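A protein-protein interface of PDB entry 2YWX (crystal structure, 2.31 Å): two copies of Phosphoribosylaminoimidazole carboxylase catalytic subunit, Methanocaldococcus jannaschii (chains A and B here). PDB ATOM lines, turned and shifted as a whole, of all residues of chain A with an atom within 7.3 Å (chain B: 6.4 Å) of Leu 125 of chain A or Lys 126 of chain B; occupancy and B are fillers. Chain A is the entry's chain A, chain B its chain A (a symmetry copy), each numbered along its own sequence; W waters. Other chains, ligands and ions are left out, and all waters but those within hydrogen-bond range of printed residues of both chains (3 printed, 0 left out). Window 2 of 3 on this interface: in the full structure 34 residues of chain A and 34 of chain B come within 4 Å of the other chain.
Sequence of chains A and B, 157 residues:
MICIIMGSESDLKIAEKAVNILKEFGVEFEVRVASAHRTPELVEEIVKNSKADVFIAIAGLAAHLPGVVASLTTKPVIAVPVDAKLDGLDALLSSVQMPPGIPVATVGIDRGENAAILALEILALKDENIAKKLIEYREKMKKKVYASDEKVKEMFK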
ATOM      1  N   ASP A  53      32.486 -10.734   3.920  1.00  0.00           N
ATOM      2  CA  ASP A  53      33.043 -11.413   5.078  1.00  0.00           C
ATOM      3  C   ASP A  53      33.259 -12.877   4.712  1.00  0.00           C
ATOM      4  O   ASP A  53      34.068 -13.573   5.329  1.00  0.00           O
ATOM      5  CB  ASP A  53      32.081 -11.329   6.267  1.00  0.00           C
ATOM      6  CG  ASP A  53      32.479 -10.265   7.269  1.00  0.00           C
ATOM      7  OD1 ASP A  53      33.616  -9.749   7.196  1.00  0.00           O
ATOM      8  OD2 ASP A  53      31.651  -9.956   8.149  1.00  0.00           O
ATOM      9  N   ALA A 119      27.784 -20.159   4.716  1.00  0.00           N
ATOM     10  CA  ALA A 119      28.149 -18.747   4.739  1.00  0.00           C
ATOM     11  C   ALA A 119      27.276 -17.977   5.739  1.00  0.00           C
ATOM     12  O   ALA A 119      27.764 -17.098   6.454  1.00  0.00           O
ATOM     13  CB  ALA A 119      27.999 -18.157   3.333  1.00  0.00           C
ATOM     14  N   LEU A 120      25.988 -18.311   5.787  1.00  0.00           N
ATOM     15  CA  LEU A 120      25.064 -17.654   6.708  1.00  0.00           C
ATOM     16  C   LEU A 120      25.379 -18.032   8.161  1.00  0.00           C
ATOM     17  O   LEU A 120      25.270 -17.200   9.068  1.00  0.00           O
ATOM     18  CB  LEU A 120      23.624 -18.032   6.356  1.00  0.00           C
ATOM     19  CG  LEU A 120      23.085 -17.426   5.053  1.00  0.00           C
ATOM     20  CD1 LEU A 120      21.898 -18.242   4.538  1.00  0.00           C
ATOM     21  CD2 LEU A 120      22.689 -15.977   5.306  1.00  0.00           C
ATOM     22  N   GLU A 121      25.775 -19.284   8.381  1.00  0.00           N
ATOM     23  CA  GLU A 121      26.122 -19.737   9.726  1.00  0.00           C
ATOM     24  C   GLU A 121      27.330 -18.937  10.214  1.00  0.00           C
ATOM     25  O   GLU A 121      27.460 -18.652  11.402  1.00  0.00           O
ATOM     26  CB  GLU A 121      26.460 -21.241   9.733  1.00  0.00           C
ATOM     27  CG  GLU A 121      25.369 -22.152   9.161  1.00  0.00           C
ATOM     28  CD  GLU A 121      25.682 -23.633   9.343  1.00  0.00           C
ATOM     29  OE1 GLU A 121      26.877 -24.002   9.354  1.00  0.00           O
ATOM     30  OE2 GLU A 121      24.735 -24.437   9.457  1.00  0.00           O
ATOM     31  N   ILE A 122      28.218 -18.580   9.291  1.00  0.00           N
ATOM     32  CA  ILE A 122      29.398 -17.803   9.655  1.00  0.00           C
ATOM     33  C   ILE A 122      28.959 -16.379  10.006  1.00  0.00           C
ATOM     34  O   ILE A 122      29.358 -15.829  11.040  1.00  0.00           O
ATOM     35  CB  ILE A 122      30.440 -17.775   8.494  1.00  0.00           C
ATOM     36  CG1 ILE A 122      31.017 -19.177   8.272  1.00  0.00           C
ATOM     37  CG2 ILE A 122      31.562 -16.810   8.810  1.00  0.00           C
ATOM     38  CD1 ILE A 122      31.879 -19.311   7.023  1.00  0.00           C
ATOM     39  N   LEU A 123      28.126 -15.782   9.155  1.00  0.00           N
ATOM     40  CA  LEU A 123      27.653 -14.423   9.413  1.00  0.00           C
ATOM     41  C   LEU A 123      26.822 -14.359  10.687  1.00  0.00           C
ATOM     42  O   LEU A 123      26.903 -13.385  11.435  1.00  0.00           O
ATOM     43  CB  LEU A 123      26.816 -13.903   8.244  1.00  0.00           C
ATOM     44  CG  LEU A 123      27.501 -13.793   6.886  1.00  0.00           C
ATOM     45  CD1 LEU A 123      26.514 -13.236   5.882  1.00  0.00           C
ATOM     46  CD2 LEU A 123      28.735 -12.891   6.986  1.00  0.00           C
ATOM     47  N   ALA A 124      26.027 -15.398  10.927  1.00  0.00           N
ATOM     48  CA  ALA A 124      25.160 -15.460  12.105  1.00  0.00           C
ATOM     49  C   ALA A 124      25.898 -15.264  13.426  1.00  0.00           C
ATOM     50  O   ALA A 124      25.290 -14.936  14.448  1.00  0.00           O
ATOM     51  CB  ALA A 124      24.392 -16.788  12.127  1.00  0.00           C
ATOM     52  N   LEU A 125      27.207 -15.480  13.407  1.00  0.00           N
ATOM     53  CA  LEU A 125      28.021 -15.310  14.603  1.00  0.00           C
ATOM     54  C   LEU A 125      28.097 -13.837  14.997  1.00  0.00           C
ATOM     55  O   LEU A 125      28.421 -13.500  16.132  1.00  0.00           O
ATOM     56  CB  LEU A 125      29.431 -15.837  14.348  1.00  0.00           C
ATOM     57  CG  LEU A 125      29.526 -17.327  14.039  1.00  0.00           C
ATOM     58  CD1 LEU A 125      30.937 -17.664  13.592  1.00  0.00           C
ATOM     59  CD2 LEU A 125      29.143 -18.123  15.275  1.00  0.00           C
ATOM     60  N   LYS A 126      27.787 -12.960  14.049  1.00  0.00           N
ATOM     61  CA  LYS A 126      27.839 -11.522  14.288  1.00  0.00           C
ATOM     62  C   LYS A 126      26.473 -10.863  14.096  1.00  0.00           C
ATOM     63  O   LYS A 126      26.202  -9.810  14.664  1.00  0.00           O
ATOM     64  CB  LYS A 126      28.862 -10.903  13.339  1.00  0.00           C
ATOM     65  CG  LYS A 126      29.355  -9.528  13.724  1.00  0.00           C
ATOM     66  CD  LYS A 126      30.569  -9.172  12.873  1.00  0.00           C
ATOM     67  CE  LYS A 126      31.110  -7.792  13.203  1.00  0.00           C
ATOM     68  NZ  LYS A 126      32.272  -7.442  12.341  1.00  0.00           N
ATOM     69  N   ASP A 127      25.621 -11.498  13.299  1.00  0.00           N
ATOM     70  CA  ASP A 127      24.277 -10.997  13.009  1.00  0.00           C
ATOM     71  C   ASP A 127      23.245 -11.914  13.663  1.00  0.00           C
ATOM     72  O   ASP A 127      22.994 -13.015  13.169  1.00  0.00           O
ATOM     73  CB  ASP A 127      24.047 -10.978  11.492  1.00  0.00           C
ATOM     74  CG  ASP A 127      22.759 -10.266  11.091  1.00  0.00           C
ATOM     75  OD1 ASP A 127      21.754 -10.355  11.835  1.00  0.00           O
ATOM     76  OD2 ASP A 127      22.744  -9.630  10.011  1.00  0.00           O
ATOM     77  N   GLU A 128      22.651 -11.468  14.767  1.00  0.00           N
ATOM     78  CA  GLU A 128      21.648 -12.268  15.466  1.00  0.00           C
ATOM     79  C   GLU A 128      20.381 -12.498  14.647  1.00  0.00           C
ATOM     80  O   GLU A 128      19.672 -13.479  14.860  1.00  0.00           O
ATOM     81  CB  GLU A 128      21.291 -11.622  16.803  1.00  0.00           C
ATOM     82  CG  GLU A 128      22.315 -11.893  17.889  1.00  0.00           C
ATOM     83  CD  GLU A 128      22.083 -11.058  19.133  1.00  0.00           C
ATOM     84  OE1 GLU A 128      20.946 -11.072  19.660  1.00  0.00           O
ATOM     85  OE2 GLU A 128      23.039 -10.390  19.584  1.00  0.00           O
ATOM     86  N   ILE A 130      20.356 -13.228  11.546  1.00  0.00           N
ATOM     87  CA  ILE A 130      20.653 -14.386  10.713  1.00  0.00           C
ATOM     88  C   ILE A 130      20.635 -15.674  11.543  1.00  0.00           C
ATOM     89  O   ILE A 130      20.138 -16.710  11.090  1.00  0.00           O
ATOM     90  CB  ILE A 130      22.021 -14.220  10.008  1.00  0.00           C
ATOM     91  CG1 ILE A 130      21.929 -13.080   8.989  1.00  0.00           C
ATOM     92  CG2 ILE A 130      22.414 -15.512   9.302  1.00  0.00           C
ATOM     93  CD1 ILE A 130      23.223 -12.794   8.257  1.00  0.00           C
ATOM     94  N   ALA A 131      21.167 -15.599  12.761  1.00  0.00           N
ATOM     95  CA  ALA A 131      21.190 -16.750  13.652  1.00  0.00           C
ATOM     96  C   ALA A 131      19.753 -17.240  13.877  1.00  0.00           C
ATOM     97  O   ALA A 131      19.455 -18.436  13.801  1.00  0.00           O
ATOM     98  CB  ALA A 131      21.826 -16.358  14.980  1.00  0.00           C
ATOM     99  N   LEU A 134      18.363 -18.990  10.889  1.00  0.00           N
ATOM    100  CA  LEU A 134      18.948 -20.318  10.711  1.00  0.00           C
ATOM    101  C   LEU A 134      18.161 -21.355  11.511  1.00  0.00           C
ATOM    102  O   LEU A 134      17.871 -22.452  11.028  1.00  0.00           O
ATOM    103  CB  LEU A 134      20.415 -20.317  11.159  1.00  0.00           C
ATOM    104  CG  LEU A 134      21.394 -19.607  10.217  1.00  0.00           C
ATOM    105  CD1 LEU A 134      22.749 -19.447  10.883  1.00  0.00           C
ATOM    106  CD2 LEU A 134      21.507 -20.407   8.926  1.00  0.00           C
ATOM    107  N   ALA B  52      31.234 -22.456  22.221  1.00  0.00           N
ATOM    108  CA  ALA B  52      32.068 -22.289  21.039  1.00  0.00           C
ATOM    109  C   ALA B  52      31.326 -21.707  19.850  1.00  0.00           C
ATOM    110  O   ALA B  52      30.163 -22.018  19.611  1.00  0.00           O
ATOM    111  CB  ALA B  52      32.695 -23.619  20.649  1.00  0.00           C
ATOM    112  N   ASP B  53      32.022 -20.846  19.115  1.00  0.00           N
ATOM    113  CA  ASP B  53      31.476 -20.221  17.921  1.00  0.00           C
ATOM    114  C   ASP B  53      31.783 -21.121  16.730  1.00  0.00           C
ATOM    115  O   ASP B  53      31.115 -21.057  15.697  1.00  0.00           O
ATOM    116  CB  ASP B  53      32.116 -18.849  17.692  1.00  0.00           C
ATOM    117  CG  ASP B  53      31.229 -17.706  18.144  1.00  0.00           C
ATOM    118  OD1 ASP B  53      30.027 -17.931  18.408  1.00  0.00           O
ATOM    119  OD2 ASP B  53      31.737 -16.570  18.216  1.00  0.00           O
ATOM    120  N   VAL B  54      32.806 -21.960  16.887  1.00  0.00           N
ATOM    121  CA  VAL B  54      33.215 -22.875  15.827  1.00  0.00           C
ATOM    122  C   VAL B  54      33.553 -24.255  16.388  1.00  0.00           C
ATOM    123  O   VAL B  54      34.233 -24.366  17.408  1.00  0.00           O
ATOM    124  CB  VAL B  54      34.458 -22.334  15.057  1.00  0.00           C
ATOM    125  CG1 VAL B  54      34.827 -23.294  13.925  1.00  0.00           C
ATOM    126  CG2 VAL B  54      34.176 -20.945  14.495  1.00  0.00           C
ATOM    127  N   THR B  74      23.894 -24.750  14.923  1.00  0.00           N
ATOM    128  CA  THR B  74      23.870 -23.962  13.695  1.00  0.00           C
ATOM    129  C   THR B  74      25.228 -23.262  13.555  1.00  0.00           C
ATOM    130  O   THR B  74      25.463 -22.514  12.605  1.00  0.00           O
ATOM    131  CB  THR B  74      22.723 -22.908  13.688  1.00  0.00           C
ATOM    132  OG1 THR B  74      22.804 -22.077  14.853  1.00  0.00           O
ATOM    133  CG2 THR B  74      21.386 -23.603  13.664  1.00  0.00           C
ATOM    134  N   LYS B  75      26.119 -23.510  14.513  1.00  0.00           N
ATOM    135  CA  LYS B  75      27.457 -22.928  14.461  1.00  0.00           C
ATOM    136  C   LYS B  75      28.218 -23.672  13.372  1.00  0.00           C
ATOM    137  O   LYS B  75      27.890 -24.814  13.044  1.00  0.00           O
ATOM    138  CB  LYS B  75      28.212 -23.125  15.778  1.00  0.00           C
ATOM    139  CG  LYS B  75      27.595 -22.486  16.990  1.00  0.00           C
ATOM    140  CD  LYS B  75      27.764 -20.980  17.002  1.00  0.00           C
ATOM    141  CE  LYS B  75      27.044 -20.398  18.212  1.00  0.00           C
ATOM    142  NZ  LYS B  75      27.233 -18.943  18.355  1.00  0.00           N
ATOM    143  N   PRO B  76      29.244 -23.025  12.793  1.00  0.00           N
ATOM    144  CA  PRO B  76      30.047 -23.649  11.742  1.00  0.00           C
ATOM    145  C   PRO B  76      30.748 -24.893  12.287  1.00  0.00           C
ATOM    146  O   PRO B  76      31.342 -24.865  13.364  1.00  0.00           O
ATOM    147  CB  PRO B  76      31.035 -22.551  11.375  1.00  0.00           C
ATOM    148  CG  PRO B  76      30.253 -21.304  11.626  1.00  0.00           C
ATOM    149  CD  PRO B  76      29.599 -21.603  12.942  1.00  0.00           C
ATOM    150  N   GLU B 121      39.964 -17.860  10.989  1.00  0.00           N
ATOM    151  CA  GLU B 121      39.511 -16.926   9.960  1.00  0.00           C
ATOM    152  C   GLU B 121      38.047 -16.575  10.231  1.00  0.00           C
ATOM    153  O   GLU B 121      37.608 -15.459   9.966  1.00  0.00           O
ATOM    154  CB  GLU B 121      39.643 -17.546   8.555  1.00  0.00           C
ATOM    155  CG  GLU B 121      41.046 -18.046   8.197  1.00  0.00           C
ATOM    156  CD  GLU B 121      41.160 -18.494   6.744  1.00  0.00           C
ATOM    157  OE1 GLU B 121      40.153 -18.969   6.177  1.00  0.00           O
ATOM    158  OE2 GLU B 121      42.263 -18.389   6.169  1.00  0.00           O
ATOM    159  N   ILE B 122      37.294 -17.536  10.756  1.00  0.00           N
ATOM    160  CA  ILE B 122      35.888 -17.294  11.064  1.00  0.00           C
ATOM    161  C   ILE B 122      35.804 -16.354  12.270  1.00  0.00           C
ATOM    162  O   ILE B 122      35.064 -15.363  12.250  1.00  0.00           O
ATOM    163  CB  ILE B 122      35.135 -18.627  11.364  1.00  0.00           C
ATOM    164  CG1 ILE B 122      35.058 -19.485  10.098  1.00  0.00           C
ATOM    165  CG2 ILE B 122      33.736 -18.344  11.871  1.00  0.00           C
ATOM    166  CD1 ILE B 122      34.539 -20.898  10.327  1.00  0.00           C
ATOM    167  N   LEU B 123      36.570 -16.654  13.316  1.00  0.00           N
ATOM    168  CA  LEU B 123      36.555 -15.809  14.510  1.00  0.00           C
ATOM    169  C   LEU B 123      37.062 -14.408  14.202  1.00  0.00           C
ATOM    170  O   LEU B 123      36.548 -13.427  14.740  1.00  0.00           O
ATOM    171  CB  LEU B 123      37.412 -16.417  15.621  1.00  0.00           C
ATOM    172  CG  LEU B 123      37.007 -17.790  16.147  1.00  0.00           C
ATOM    173  CD1 LEU B 123      37.960 -18.193  17.253  1.00  0.00           C
ATOM    174  CD2 LEU B 123      35.565 -17.755  16.665  1.00  0.00           C
ATOM    175  N   ALA B 124      38.067 -14.319  13.336  1.00  0.00           N
ATOM    176  CA  ALA B 124      38.664 -13.035  12.963  1.00  0.00           C
ATOM    177  C   ALA B 124      37.656 -12.013  12.443  1.00  0.00           C
ATOM    178  O   ALA B 124      37.925 -10.809  12.431  1.00  0.00           O
ATOM    179  CB  ALA B 124      39.774 -13.249  11.925  1.00  0.00           C
ATOM    180  N   LEU B 125      36.502 -12.496  12.002  1.00  0.00           N
ATOM    181  CA  LEU B 125      35.456 -11.618  11.497  1.00  0.00           C
ATOM    182  C   LEU B 125      34.868 -10.777  12.628  1.00  0.00           C
ATOM    183  O   LEU B 125      34.241  -9.747  12.393  1.00  0.00           O
ATOM    184  CB  LEU B 125      34.347 -12.449  10.857  1.00  0.00           C
ATOM    185  CG  LEU B 125      34.764 -13.271   9.643  1.00  0.00           C
ATOM    186  CD1 LEU B 125      33.635 -14.207   9.251  1.00  0.00           C
ATOM    187  CD2 LEU B 125      35.116 -12.336   8.499  1.00  0.00           C
ATOM    188  N   LYS B 126      35.082 -11.220  13.861  1.00  0.00           N
ATOM    189  CA  LYS B 126      34.557 -10.523  15.029  1.00  0.00           C
ATOM    190  C   LYS B 126      35.673 -10.055  15.963  1.00  0.00           C
ATOM    191  O   LYS B 126      35.501  -9.103  16.716  1.00  0.00           O
ATOM    192  CB  LYS B 126      33.603 -11.456  15.771  1.00  0.00           C
ATOM    193  CG  LYS B 126      32.656 -10.781  16.736  1.00  0.00           C
ATOM    194  CD  LYS B 126      31.584 -11.776  17.167  1.00  0.00           C
ATOM    195  CE  LYS B 126      30.602 -11.163  18.150  1.00  0.00           C
ATOM    196  NZ  LYS B 126      29.582 -12.154  18.589  1.00  0.00           N
ATOM    197  N   ASP B 127      36.816 -10.731  15.897  1.00  0.00           N
ATOM    198  CA  ASP B 127      37.978 -10.413  16.727  1.00  0.00           C
ATOM    199  C   ASP B 127      39.087  -9.843  15.843  1.00  0.00           C
ATOM    200  O   ASP B 127      39.748 -10.591  15.120  1.00  0.00           O
ATOM    201  CB  ASP B 127      38.486 -11.685  17.418  1.00  0.00           C
ATOM    202  CG  ASP B 127      39.555 -11.408  18.470  1.00  0.00           C
ATOM    203  OD1 ASP B 127      40.373 -10.478  18.280  1.00  0.00           O
ATOM    204  OD2 ASP B 127      39.592 -12.141  19.486  1.00  0.00           O
ATOM    205  N   GLU B 128      39.292  -8.529  15.899  1.00  0.00           N
ATOM    206  CA  GLU B 128      40.329  -7.887  15.096  1.00  0.00           C
ATOM    207  C   GLU B 128      41.742  -8.317  15.480  1.00  0.00           C
ATOM    208  O   GLU B 128      42.656  -8.258  14.660  1.00  0.00           O
ATOM    209  CB  GLU B 128      40.207  -6.368  15.185  1.00  0.00           C
ATOM    210  CG  GLU B 128      39.118  -5.803  14.293  1.00  0.00           C
ATOM    211  CD  GLU B 128      38.841  -4.337  14.564  1.00  0.00           C
ATOM    212  OE1 GLU B 128      39.803  -3.535  14.556  1.00  0.00           O
ATOM    213  OE2 GLU B 128      37.659  -3.989  14.783  1.00  0.00           O
HETATM  214  O   HOH W   1      27.894 -15.802  18.465  1.00  0.00           O
HETATM  215  O   HOH W   2      26.167 -19.692  13.465  1.00  0.00           O
HETATM  216  O   HOH W   3      34.962  -8.319   9.484  1.00  0.00           O
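The side-chain amino group (NZ) of Lys 126 of chain A lies within hydrogen-bond range of the backbone carbonyl oxygen (O) of Leu 125 of chain B (3.0 Å).
The side-chain amino group (NZ) of Lys 126 of chain B sits at hydrogen-bond distance from the backbone carbonyl oxygen (O) of Leu 125 of chain A, at 3.0 Å.
The side-chain carboxylate (OD1) of Asp 53 of chain B is in salt-bridge range of the side-chain amino group (NZ) of Lys 75 of chain B (3.0 Å).
OD1 of Asp 53 of chain A touches CD2 of Leu 125 of chain B, 3.3 Å away.
CB of Glu 121 of chain A touches O of Thr 74 of chain B, at 3.3 Å.
O of Lys 75 of chain B touches OE1 of Glu 121 of chain A (3.9 Å).
Glu 121 of chain A touches Pro 76 of chain B.
CG2 of Ile 122 of chain A touches CD1 of Leu 125 of chain B (3.4 Å).
Asp 53 of chain B touches Leu 125 of chain A (OD1 to CD2, 3.3 Å).
Leu 125 of chain A touches Lys 75 of chain B (CD2 to CD, 3.6 Å).
Ile 122 of chain B touches Leu 125 of chain A.
Of the printed residues of chain B, Leu 125 of chain A touches Asp 53 (3.3 Å), Lys 75 (3.6 Å), Ile 122 (3.4 Å) and Lys 126 (3.0 Å).
Lys 126 of chain B touches one residue of chain A.
Printed residues of chain A within 4 Å of Leu 125 of chain B: Asp 53 (3.3 Å), Ile 122 (3.4 Å) and Lys 126 (3.0 Å).
Printed residues of chain A within 4 Å of Pro 76 of chain B: Glu 121 (3.9 Å).
Printed residues of chain A within 4 Å of Asp 53 of chain B: Leu 125 (3.3 Å).
Ala 124 of chain B touches none of the printed residues of chain A.
The nearest residue of chain B that does not touch Leu 125 of chain A is Pro 76 of chain B (4.2 Å).
The nearest residue of chain A that does not touch Lys 126 of chain B is Lys 126 of chain A (4.6 Å).
Among the printed residues, 10 pairs touch across the chains.
Among the printed residues, no Asp or Glu carboxylate lies within 4 Å of a Lys or Arg side-chain nitrogen of the other chain.
Asp 53 of chain A touches Leu 125 of chain B, and with the chains exchanged Leu 125 of chain A touches Asp 53 of chain B.
Ile 122 of chain A touches Leu 125 of chain B, and with the chains exchanged Leu 125 of chain A touches Ile 122 of chain B.
Leu 125 of chain A touches Lys 126 of chain B, and with the chains exchanged Lys 126 of chain A touches Leu 125 of chain B.
Positions printed for both chains: 53, 121, 122, 123, 124, 125, 126, 127 and 128.
Of the 10 pairs that touch across the chains among the printed residues, 6 have their exchanged pair printed and touching as well.
Water W2 lies within hydrogen-bond range of the backbone carbonyl oxygen (O) of Glu 121 of chain A and the backbone carbonyl oxygen (O) of Thr 74 of chain B.
Water W3 bridges OD1 of Asp 53 of chain A (3.0 Å) and O of Leu 125 of chain B (3.3 Å).
Water W1 lies within hydrogen-bond range of the side-chain carboxylate of Asp 53 of chain B (3.0 Å), the side-chain amino group of Lys 75 of chain B (3.2 Å) and the backbone carbonyl oxygen of Leu 125 of chain A (3.3 Å).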
